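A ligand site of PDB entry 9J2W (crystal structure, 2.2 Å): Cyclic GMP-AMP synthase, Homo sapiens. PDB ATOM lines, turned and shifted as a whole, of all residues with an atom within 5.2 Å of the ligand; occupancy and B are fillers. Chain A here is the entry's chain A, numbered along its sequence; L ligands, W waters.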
ATOM      1  N   VAL A  62      10.209 -23.603  14.786  1.00  0.00           N
ATOM      2  CA  VAL A  62      10.876 -23.218  13.547  1.00  0.00           C
ATOM      3  C   VAL A  62      10.917 -21.701  13.415  1.00  0.00           C
ATOM      4  O   VAL A  62      11.944 -21.128  13.037  1.00  0.00           O
ATOM      5  CB  VAL A  62      10.162 -23.871  12.352  1.00  0.00           C
ATOM      6  CG1 VAL A  62      10.669 -23.283  11.065  1.00  0.00           C
ATOM      7  CG2 VAL A  62      10.384 -25.377  12.377  1.00  0.00           C
ATOM      8  N   LYS A  63       9.806 -21.031  13.725  1.00  0.00           N
ATOM      9  CA  LYS A  63       9.750 -19.579  13.725  1.00  0.00           C
ATOM     10  C   LYS A  63       9.793 -19.098  15.169  1.00  0.00           C
ATOM     11  O   LYS A  63       8.956 -19.485  15.983  1.00  0.00           O
ATOM     12  CB  LYS A  63       8.477 -19.092  13.034  1.00  0.00           C
ATOM     13  CG  LYS A  63       8.200 -19.738  11.684  1.00  0.00           C
ATOM     14  CD  LYS A  63       6.804 -19.410  11.175  1.00  0.00           C
ATOM     15  CE  LYS A  63       6.301 -18.076  11.730  1.00  0.00           C
ATOM     16  NZ  LYS A  63       5.082 -17.594  11.011  1.00  0.00           N
ATOM     17  N   ASP A  71       7.176 -28.105  16.070  1.00  0.00           N
ATOM     18  CA  ASP A  71       7.775 -28.936  15.022  1.00  0.00           C
ATOM     19  C   ASP A  71       8.476 -30.100  15.702  1.00  0.00           C
ATOM     20  O   ASP A  71       9.458 -29.897  16.420  1.00  0.00           O
ATOM     21  CB  ASP A  71       8.752 -28.126  14.169  1.00  0.00           C
ATOM     22  CG  ASP A  71       8.767 -28.559  12.724  1.00  0.00           C
ATOM     23  OD1 ASP A  71       9.536 -29.479  12.377  1.00  0.00           O
ATOM     24  OD2 ASP A  71       8.000 -27.982  11.921  1.00  0.00           O
ATOM     25  N   ALA A  91      22.386 -34.272  -1.965  1.00  0.00           N
ATOM     26  CA  ALA A  91      21.495 -34.237  -0.810  1.00  0.00           C
ATOM     27  C   ALA A  91      20.290 -35.163  -0.912  1.00  0.00           C
ATOM     28  O   ALA A  91      19.714 -35.496   0.126  1.00  0.00           O
ATOM     29  CB  ALA A  91      21.003 -32.804  -0.561  1.00  0.00           C
ATOM     30  N   SER A 149       7.499 -33.509   3.692  1.00  0.00           N
ATOM     31  CA  SER A 149       7.986 -33.371   5.056  1.00  0.00           C
ATOM     32  C   SER A 149       7.514 -32.051   5.675  1.00  0.00           C
ATOM     33  O   SER A 149       6.663 -32.045   6.583  1.00  0.00           O
ATOM     34  CB  SER A 149       9.517 -33.445   5.113  1.00  0.00           C
ATOM     35  OG  SER A 149       9.975 -34.775   4.942  1.00  0.00           O
ATOM     36  N   THR A 165       6.926 -34.578  10.988  1.00  0.00           N
ATOM     37  CA  THR A 165       7.760 -35.053   9.893  1.00  0.00           C
ATOM     38  C   THR A 165       8.248 -36.459  10.226  1.00  0.00           C
ATOM     39  O   THR A 165       8.699 -36.715  11.358  1.00  0.00           O
ATOM     40  CB  THR A 165       8.989 -34.156   9.729  1.00  0.00           C
ATOM     41  OG1 THR A 165       8.589 -32.840   9.332  1.00  0.00           O
ATOM     42  CG2 THR A 165       9.981 -34.721   8.718  1.00  0.00           C
ATOM     43  N   LYS A 206      11.232 -36.201   0.625  1.00  0.00           N
ATOM     44  CA  LYS A 206      11.167 -34.889  -0.012  1.00  0.00           C
ATOM     45  C   LYS A 206      11.371 -35.019  -1.506  1.00  0.00           C
ATOM     46  O   LYS A 206      12.271 -35.735  -1.960  1.00  0.00           O
ATOM     47  CB  LYS A 206      12.202 -33.935   0.589  1.00  0.00           C
ATOM     48  CG  LYS A 206      11.876 -32.472   0.361  1.00  0.00           C
ATOM     49  CD  LYS A 206      11.535 -31.786   1.667  1.00  0.00           C
ATOM     50  CE  LYS A 206      10.614 -30.604   1.427  1.00  0.00           C
ATOM     51  NZ  LYS A 206       9.897 -30.215   2.676  1.00  0.00           N
ATOM     52  N   ARG A 220      15.818 -36.909   1.601  1.00  0.00           N
ATOM     53  CA  ARG A 220      16.809 -35.850   1.731  1.00  0.00           C
ATOM     54  C   ARG A 220      17.494 -35.932   3.086  1.00  0.00           C
ATOM     55  O   ARG A 220      16.850 -36.177   4.108  1.00  0.00           O
ATOM     56  CB  ARG A 220      16.171 -34.467   1.553  1.00  0.00           C
ATOM     57  CG  ARG A 220      17.186 -33.337   1.547  1.00  0.00           C
ATOM     58  CD  ARG A 220      16.538 -32.001   1.225  1.00  0.00           C
ATOM     59  NE  ARG A 220      15.759 -31.492   2.353  1.00  0.00           N
ATOM     60  CZ  ARG A 220      14.913 -30.478   2.272  1.00  0.00           C
ATOM     61  NH1 ARG A 220      14.707 -29.828   1.137  1.00  0.00           N
ATOM     62  NH2 ARG A 220      14.250 -30.091   3.366  1.00  0.00           N
ATOM     63  N   LEU A 221      18.807 -35.708   3.071  1.00  0.00           N
ATOM     64  CA  LEU A 221      19.613 -35.774   4.291  1.00  0.00           C
ATOM     65  C   LEU A 221      19.187 -34.711   5.284  1.00  0.00           C
ATOM     66  O   LEU A 221      18.889 -33.575   4.924  1.00  0.00           O
ATOM     67  CB  LEU A 221      21.090 -35.617   3.940  1.00  0.00           C
ATOM     68  CG  LEU A 221      21.757 -36.842   3.323  1.00  0.00           C
ATOM     69  CD1 LEU A 221      23.207 -36.544   2.991  1.00  0.00           C
ATOM     70  CD2 LEU A 221      21.671 -38.022   4.280  1.00  0.00           C
ATOM     71  N   LEU A 261      14.367 -12.182   9.353  1.00  0.00           N
ATOM     72  CA  LEU A 261      13.788 -12.835   8.180  1.00  0.00           C
ATOM     73  C   LEU A 261      12.294 -13.053   8.340  1.00  0.00           C
ATOM     74  O   LEU A 261      11.527 -12.878   7.392  1.00  0.00           O
ATOM     75  CB  LEU A 261      14.485 -14.175   7.893  1.00  0.00           C
ATOM     76  CG  LEU A 261      13.905 -14.866   6.658  1.00  0.00           C
ATOM     77  CD1 LEU A 261      14.071 -13.992   5.422  1.00  0.00           C
ATOM     78  CD2 LEU A 261      14.530 -16.230   6.441  1.00  0.00           C
ATOM     79  N   GLU A 262      11.846 -13.445   9.544  1.00  0.00           N
ATOM     80  CA  GLU A 262      10.418 -13.683   9.752  1.00  0.00           C
ATOM     81  C   GLU A 262       9.611 -12.401   9.587  1.00  0.00           C
ATOM     82  O   GLU A 262       8.561 -12.408   8.925  1.00  0.00           O
ATOM     83  CB  GLU A 262      10.187 -14.292  11.136  1.00  0.00           C
ATOM     84  CG  GLU A 262      10.703 -15.715  11.271  1.00  0.00           C
ATOM     85  CD  GLU A 262      10.731 -16.191  12.705  1.00  0.00           C
ATOM     86  OE1 GLU A 262       9.915 -15.693  13.511  1.00  0.00           O
ATOM     87  OE2 GLU A 262      11.571 -17.058  13.041  1.00  0.00           O
ATOM     88  N   LYS A 265       9.467 -11.501   5.913  1.00  0.00           N
ATOM     89  CA  LYS A 265       8.565 -12.391   5.186  1.00  0.00           C
ATOM     90  C   LYS A 265       7.108 -12.038   5.458  1.00  0.00           C
ATOM     91  O   LYS A 265       6.269 -12.081   4.546  1.00  0.00           O
ATOM     92  CB  LYS A 265       8.837 -13.852   5.568  1.00  0.00           C
ATOM     93  CG  LYS A 265      10.051 -14.456   4.879  1.00  0.00           C
ATOM     94  CD  LYS A 265      10.426 -15.796   5.506  1.00  0.00           C
ATOM     95  CE  LYS A 265       9.471 -16.899   5.073  1.00  0.00           C
ATOM     96  NZ  LYS A 265       9.756 -17.356   3.689  1.00  0.00           N
ATOM     97  N   PHE A 277      12.736 -18.129   1.004  1.00  0.00           N
ATOM     98  CA  PHE A 277      13.726 -18.017   2.071  1.00  0.00           C
ATOM     99  C   PHE A 277      13.168 -18.576   3.361  1.00  0.00           C
ATOM    100  O   PHE A 277      11.966 -18.479   3.647  1.00  0.00           O
ATOM    101  CB  PHE A 277      14.137 -16.557   2.259  1.00  0.00           C
ATOM    102  CG  PHE A 277      14.782 -15.953   1.049  1.00  0.00           C
ATOM    103  CD1 PHE A 277      16.114 -16.218   0.745  1.00  0.00           C
ATOM    104  CD2 PHE A 277      14.057 -15.128   0.201  1.00  0.00           C
ATOM    105  CE1 PHE A 277      16.699 -15.660  -0.373  1.00  0.00           C
ATOM    106  CE2 PHE A 277      14.646 -14.572  -0.926  1.00  0.00           C
ATOM    107  CZ  PHE A 277      15.978 -14.838  -1.208  1.00  0.00           C
ATOM    108  N   SER A 278      14.045 -19.171   4.166  1.00  0.00           N
ATOM    109  CA  SER A 278      13.631 -19.841   5.389  1.00  0.00           C
ATOM    110  C   SER A 278      14.715 -19.701   6.441  1.00  0.00           C
ATOM    111  O   SER A 278      15.831 -19.239   6.173  1.00  0.00           O
ATOM    112  CB  SER A 278      13.335 -21.327   5.139  1.00  0.00           C
ATOM    113  OG  SER A 278      14.523 -22.094   5.168  1.00  0.00           O
ATOM    114  N   SER A 279      14.375 -20.112   7.668  1.00  0.00           N
ATOM    115  CA  SER A 279      15.329 -20.088   8.765  1.00  0.00           C
ATOM    116  C   SER A 279      16.488 -21.053   8.543  1.00  0.00           C
ATOM    117  O   SER A 279      17.512 -20.940   9.229  1.00  0.00           O
ATOM    118  CB  SER A 279      14.623 -20.413  10.088  1.00  0.00           C
ATOM    119  OG  SER A 279      14.292 -21.789  10.163  1.00  0.00           O
ATOM    120  N   TYR A 280      16.336 -21.996   7.612  1.00  0.00           N
ATOM    121  CA  TYR A 280      17.466 -22.873   7.291  1.00  0.00           C
ATOM    122  C   TYR A 280      18.608 -22.093   6.663  1.00  0.00           C
ATOM    123  O   TYR A 280      19.773 -22.323   6.994  1.00  0.00           O
ATOM    124  CB  TYR A 280      17.020 -24.007   6.372  1.00  0.00           C
ATOM    125  CG  TYR A 280      18.035 -25.116   6.317  1.00  0.00           C
ATOM    126  CD1 TYR A 280      18.302 -25.893   7.437  1.00  0.00           C
ATOM    127  CD2 TYR A 280      18.757 -25.378   5.151  1.00  0.00           C
ATOM    128  CE1 TYR A 280      19.236 -26.910   7.393  1.00  0.00           C
ATOM    129  CE2 TYR A 280      19.696 -26.387   5.109  1.00  0.00           C
ATOM    130  CZ  TYR A 280      19.932 -27.145   6.232  1.00  0.00           C
ATOM    131  OH  TYR A 280      20.871 -28.154   6.190  1.00  0.00           O
ATOM    132  N   ASN A 326      25.532 -25.548   1.865  1.00  0.00           N
ATOM    133  CA  ASN A 326      24.997 -26.321   2.978  1.00  0.00           C
ATOM    134  C   ASN A 326      26.136 -26.667   3.928  1.00  0.00           C
ATOM    135  O   ASN A 326      27.181 -27.170   3.510  1.00  0.00           O
ATOM    136  CB  ASN A 326      24.313 -27.584   2.460  1.00  0.00           C
ATOM    137  CG  ASN A 326      23.678 -28.414   3.567  1.00  0.00           C
ATOM    138  OD1 ASN A 326      24.369 -29.007   4.391  1.00  0.00           O
ATOM    139  ND2 ASN A 326      22.348 -28.454   3.586  1.00  0.00           N
ATOM    140  N   ILE A 329      26.786 -30.353   3.644  1.00  0.00           N
ATOM    141  CA  ILE A 329      26.943 -30.843   2.279  1.00  0.00           C
ATOM    142  C   ILE A 329      27.519 -29.708   1.441  1.00  0.00           C
ATOM    143  O   ILE A 329      26.758 -29.019   0.745  1.00  0.00           O
ATOM    144  CB  ILE A 329      25.594 -31.340   1.712  1.00  0.00           C
ATOM    145  CG1 ILE A 329      24.873 -32.204   2.748  1.00  0.00           C
ATOM    146  CG2 ILE A 329      25.809 -32.128   0.418  1.00  0.00           C
ATOM    147  CD1 ILE A 329      23.448 -32.540   2.387  1.00  0.00           C
ATOM    148  N   PHE A 332      26.355 -28.597  -2.034  1.00  0.00           N
ATOM    149  CA  PHE A 332      24.970 -28.187  -2.212  1.00  0.00           C
ATOM    150  C   PHE A 332      24.880 -26.687  -1.954  1.00  0.00           C
ATOM    151  O   PHE A 332      25.192 -26.219  -0.849  1.00  0.00           O
ATOM    152  CB  PHE A 332      24.058 -28.963  -1.276  1.00  0.00           C
ATOM    153  CG  PHE A 332      22.602 -28.895  -1.657  1.00  0.00           C
ATOM    154  CD1 PHE A 332      21.822 -27.808  -1.287  1.00  0.00           C
ATOM    155  CD2 PHE A 332      22.009 -29.919  -2.375  1.00  0.00           C
ATOM    156  CE1 PHE A 332      20.491 -27.736  -1.628  1.00  0.00           C
ATOM    157  CE2 PHE A 332      20.673 -29.856  -2.716  1.00  0.00           C
ATOM    158  CZ  PHE A 332      19.911 -28.767  -2.350  1.00  0.00           C
ATOM    159  N   LEU A 334      22.547 -23.699  -1.430  1.00  0.00           N
ATOM    160  CA  LEU A 334      21.178 -23.345  -1.103  1.00  0.00           C
ATOM    161  C   LEU A 334      20.712 -22.110  -1.871  1.00  0.00           C
ATOM    162  O   LEU A 334      19.510 -21.930  -2.086  1.00  0.00           O
ATOM    163  CB  LEU A 334      21.029 -23.121   0.402  1.00  0.00           C
ATOM    164  CG  LEU A 334      21.400 -24.282   1.314  1.00  0.00           C
ATOM    165  CD1 LEU A 334      21.622 -23.799   2.733  1.00  0.00           C
ATOM    166  CD2 LEU A 334      20.328 -25.352   1.281  1.00  0.00           C
HETATM  167  C1  LIG L   1      19.072 -30.298   4.055  1.00  0.00           C
HETATM  168  C2  LIG L   1      13.215 -24.390   8.335  1.00  0.00           C
HETATM  169  C3  LIG L   1      18.044 -29.374   3.977  1.00  0.00           C
HETATM  170  C4  LIG L   1      17.853 -28.593   2.827  1.00  0.00           C
HETATM  171  C5  LIG L   1      12.211 -26.336   6.803  1.00  0.00           C
HETATM  172  C6  LIG L   1      16.313 -28.028   4.288  1.00  0.00           C
HETATM  173  C7  LIG L   1      13.478 -26.024   4.688  1.00  0.00           C
HETATM  174  C8  LIG L   1      13.393 -26.690   5.929  1.00  0.00           C
HETATM  175  C9  LIG L   1      14.464 -27.577   5.976  1.00  0.00           C
HETATM  176  C10 LIG L   1      12.258 -24.988   7.484  1.00  0.00           C
HETATM  177  C11 LIG L   1      11.582 -27.502   7.564  1.00  0.00           C
HETATM  178  N1  LIG L   1      17.056 -29.008   4.878  1.00  0.00           N
HETATM  179  N2  LIG L   1      16.758 -27.741   3.000  1.00  0.00           N
HETATM  180  C12 LIG L   1      19.892 -30.427   2.960  1.00  0.00           C
HETATM  181  N3  LIG L   1      15.170 -27.398   4.804  1.00  0.00           N
HETATM  182  C13 LIG L   1      18.697 -28.724   1.734  1.00  0.00           C
HETATM  183  C14 LIG L   1      11.286 -24.034   7.260  1.00  0.00           C
HETATM  184  C15 LIG L   1      10.941 -21.705   8.071  1.00  0.00           C
HETATM  185  C16 LIG L   1       9.315 -20.184   7.962  1.00  0.00           C
HETATM  186  C17 LIG L   1      10.495 -19.564   8.411  1.00  0.00           C
HETATM  187  C18 LIG L   1       8.134 -19.488   7.802  1.00  0.00           C
HETATM  188  C19 LIG L   1      19.704 -29.659   1.814  1.00  0.00           C
HETATM  189  C20 LIG L   1       8.161 -18.142   8.100  1.00  0.00           C
HETATM  190  C21 LIG L   1       9.326 -17.512   8.540  1.00  0.00           C
HETATM  191  C22 LIG L   1      10.502 -18.207   8.708  1.00  0.00           C
HETATM  192  C23 LIG L   1      10.840 -29.675   7.459  1.00  0.00           C
HETATM  193  C24 LIG L   1      10.432 -29.660   8.769  1.00  0.00           C
HETATM  194  C25 LIG L   1      10.606 -28.508   9.493  1.00  0.00           C
HETATM  195  C26 LIG L   1      11.178 -27.409   8.885  1.00  0.00           C
HETATM  196  C27 LIG L   1      12.577 -24.978   4.120  1.00  0.00           C
HETATM  197  C28 LIG L   1      14.476 -24.947   8.885  1.00  0.00           C
HETATM  198  N4  LIG L   1      14.537 -26.448   4.026  1.00  0.00           N
HETATM  199  N5  LIG L   1      12.823 -23.149   8.634  1.00  0.00           N
HETATM  200  N6  LIG L   1      11.621 -22.929   7.981  1.00  0.00           N
HETATM  201  N7  LIG L   1       9.618 -21.513   7.758  1.00  0.00           N
HETATM  202  N8  LIG L   1      11.510 -20.501   8.473  1.00  0.00           N
HETATM  203  N9  LIG L   1      11.399 -28.614   6.852  1.00  0.00           N
HETATM  204  O1  LIG L   1      14.847 -28.434   6.908  1.00  0.00           O
HETATM  205  O2  LIG L   1      10.191 -24.112   6.531  1.00  0.00           O
HETATM  206  O   HOH W   1      15.320 -23.854   2.921  1.00  0.00           O
HETATM  207  O   HOH W   2      16.592 -32.385   5.114  1.00  0.00           O
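ND2 of Asn 326 is in hydrogen-bond range of OH of Tyr 280 (3.0 Å).
The backbone NH of Asn 326 is in hydrogen-bond range of the backbone carbonyl oxygen of Phe 332 (2.8 Å).
OD1 of Asn 326 sits at hydrogen-bond distance from N of Ile 329 (2.9 Å).
O of Ala 91 sits at hydrogen-bond distance from N of Leu 221 (3.1 Å).
The side-chain hydroxyl of Ser 278 lies close to the backbone NH of Tyr 280 (3.0 Å).
The side-chain amino group of Lys 265 lies within hydrogen-bond range of the backbone carbonyl oxygen of Phe 277 (2.5 Å).
OG1 of Thr 165 sits at hydrogen-bond distance from O of Ser 149 (3.4 Å).
A nitrogen (N8) of the ligand sits at hydrogen-bond distance from the backbone NH (N) of Ser 279, at 3.0 Å.
The side-chain hydroxyl (OG) of Ser 279 is in hydrogen-bond range of a nitrogen (N5) of the ligand (2.5 Å).
The guanidinium group (NH2) of Arg 220 sits close to a nitrogen (N2) of the ligand, at 3.5 Å.
Water W1 lies within hydrogen-bond range of a nitrogen (N4) of the ligand (2.9 Å) and the side-chain hydroxyl (OG) of Ser 278 (3.0 Å).
Water W2 lies within hydrogen-bond range of O of Leu 221 (2.6 Å), NE of Arg 220 (3.0 Å) and N1 of the ligand (3.4 Å).
Val 62 touches the ligand (CG1 to N6, 3.2 Å).
Lys 63 touches the ligand (CD to C20, 3.6 Å).
Asp 71 touches the ligand.
Thr 165 touches the ligand (OG1 to C24, 3.7 Å).
Leu 221 touches the ligand.
CG of Glu 262 touches C21 of the ligand (3.5 Å).
Lys 265 touches the ligand.
Ser 278 touches the ligand (OG to C27, 3.6 Å).
OH of Tyr 280 touches C1 of the ligand, 3.5 Å away.
Asn 326 touches the ligand.
Phe 332 touches the ligand.
Leu 334 touches the ligand.
Hydrophobic or aromatic side chains within 4 Å of the ligand: Val 62, Tyr 280, Phe 332 and Leu 334.
Of the 20 residues printed, 14 come within 4 Å of the ligand.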
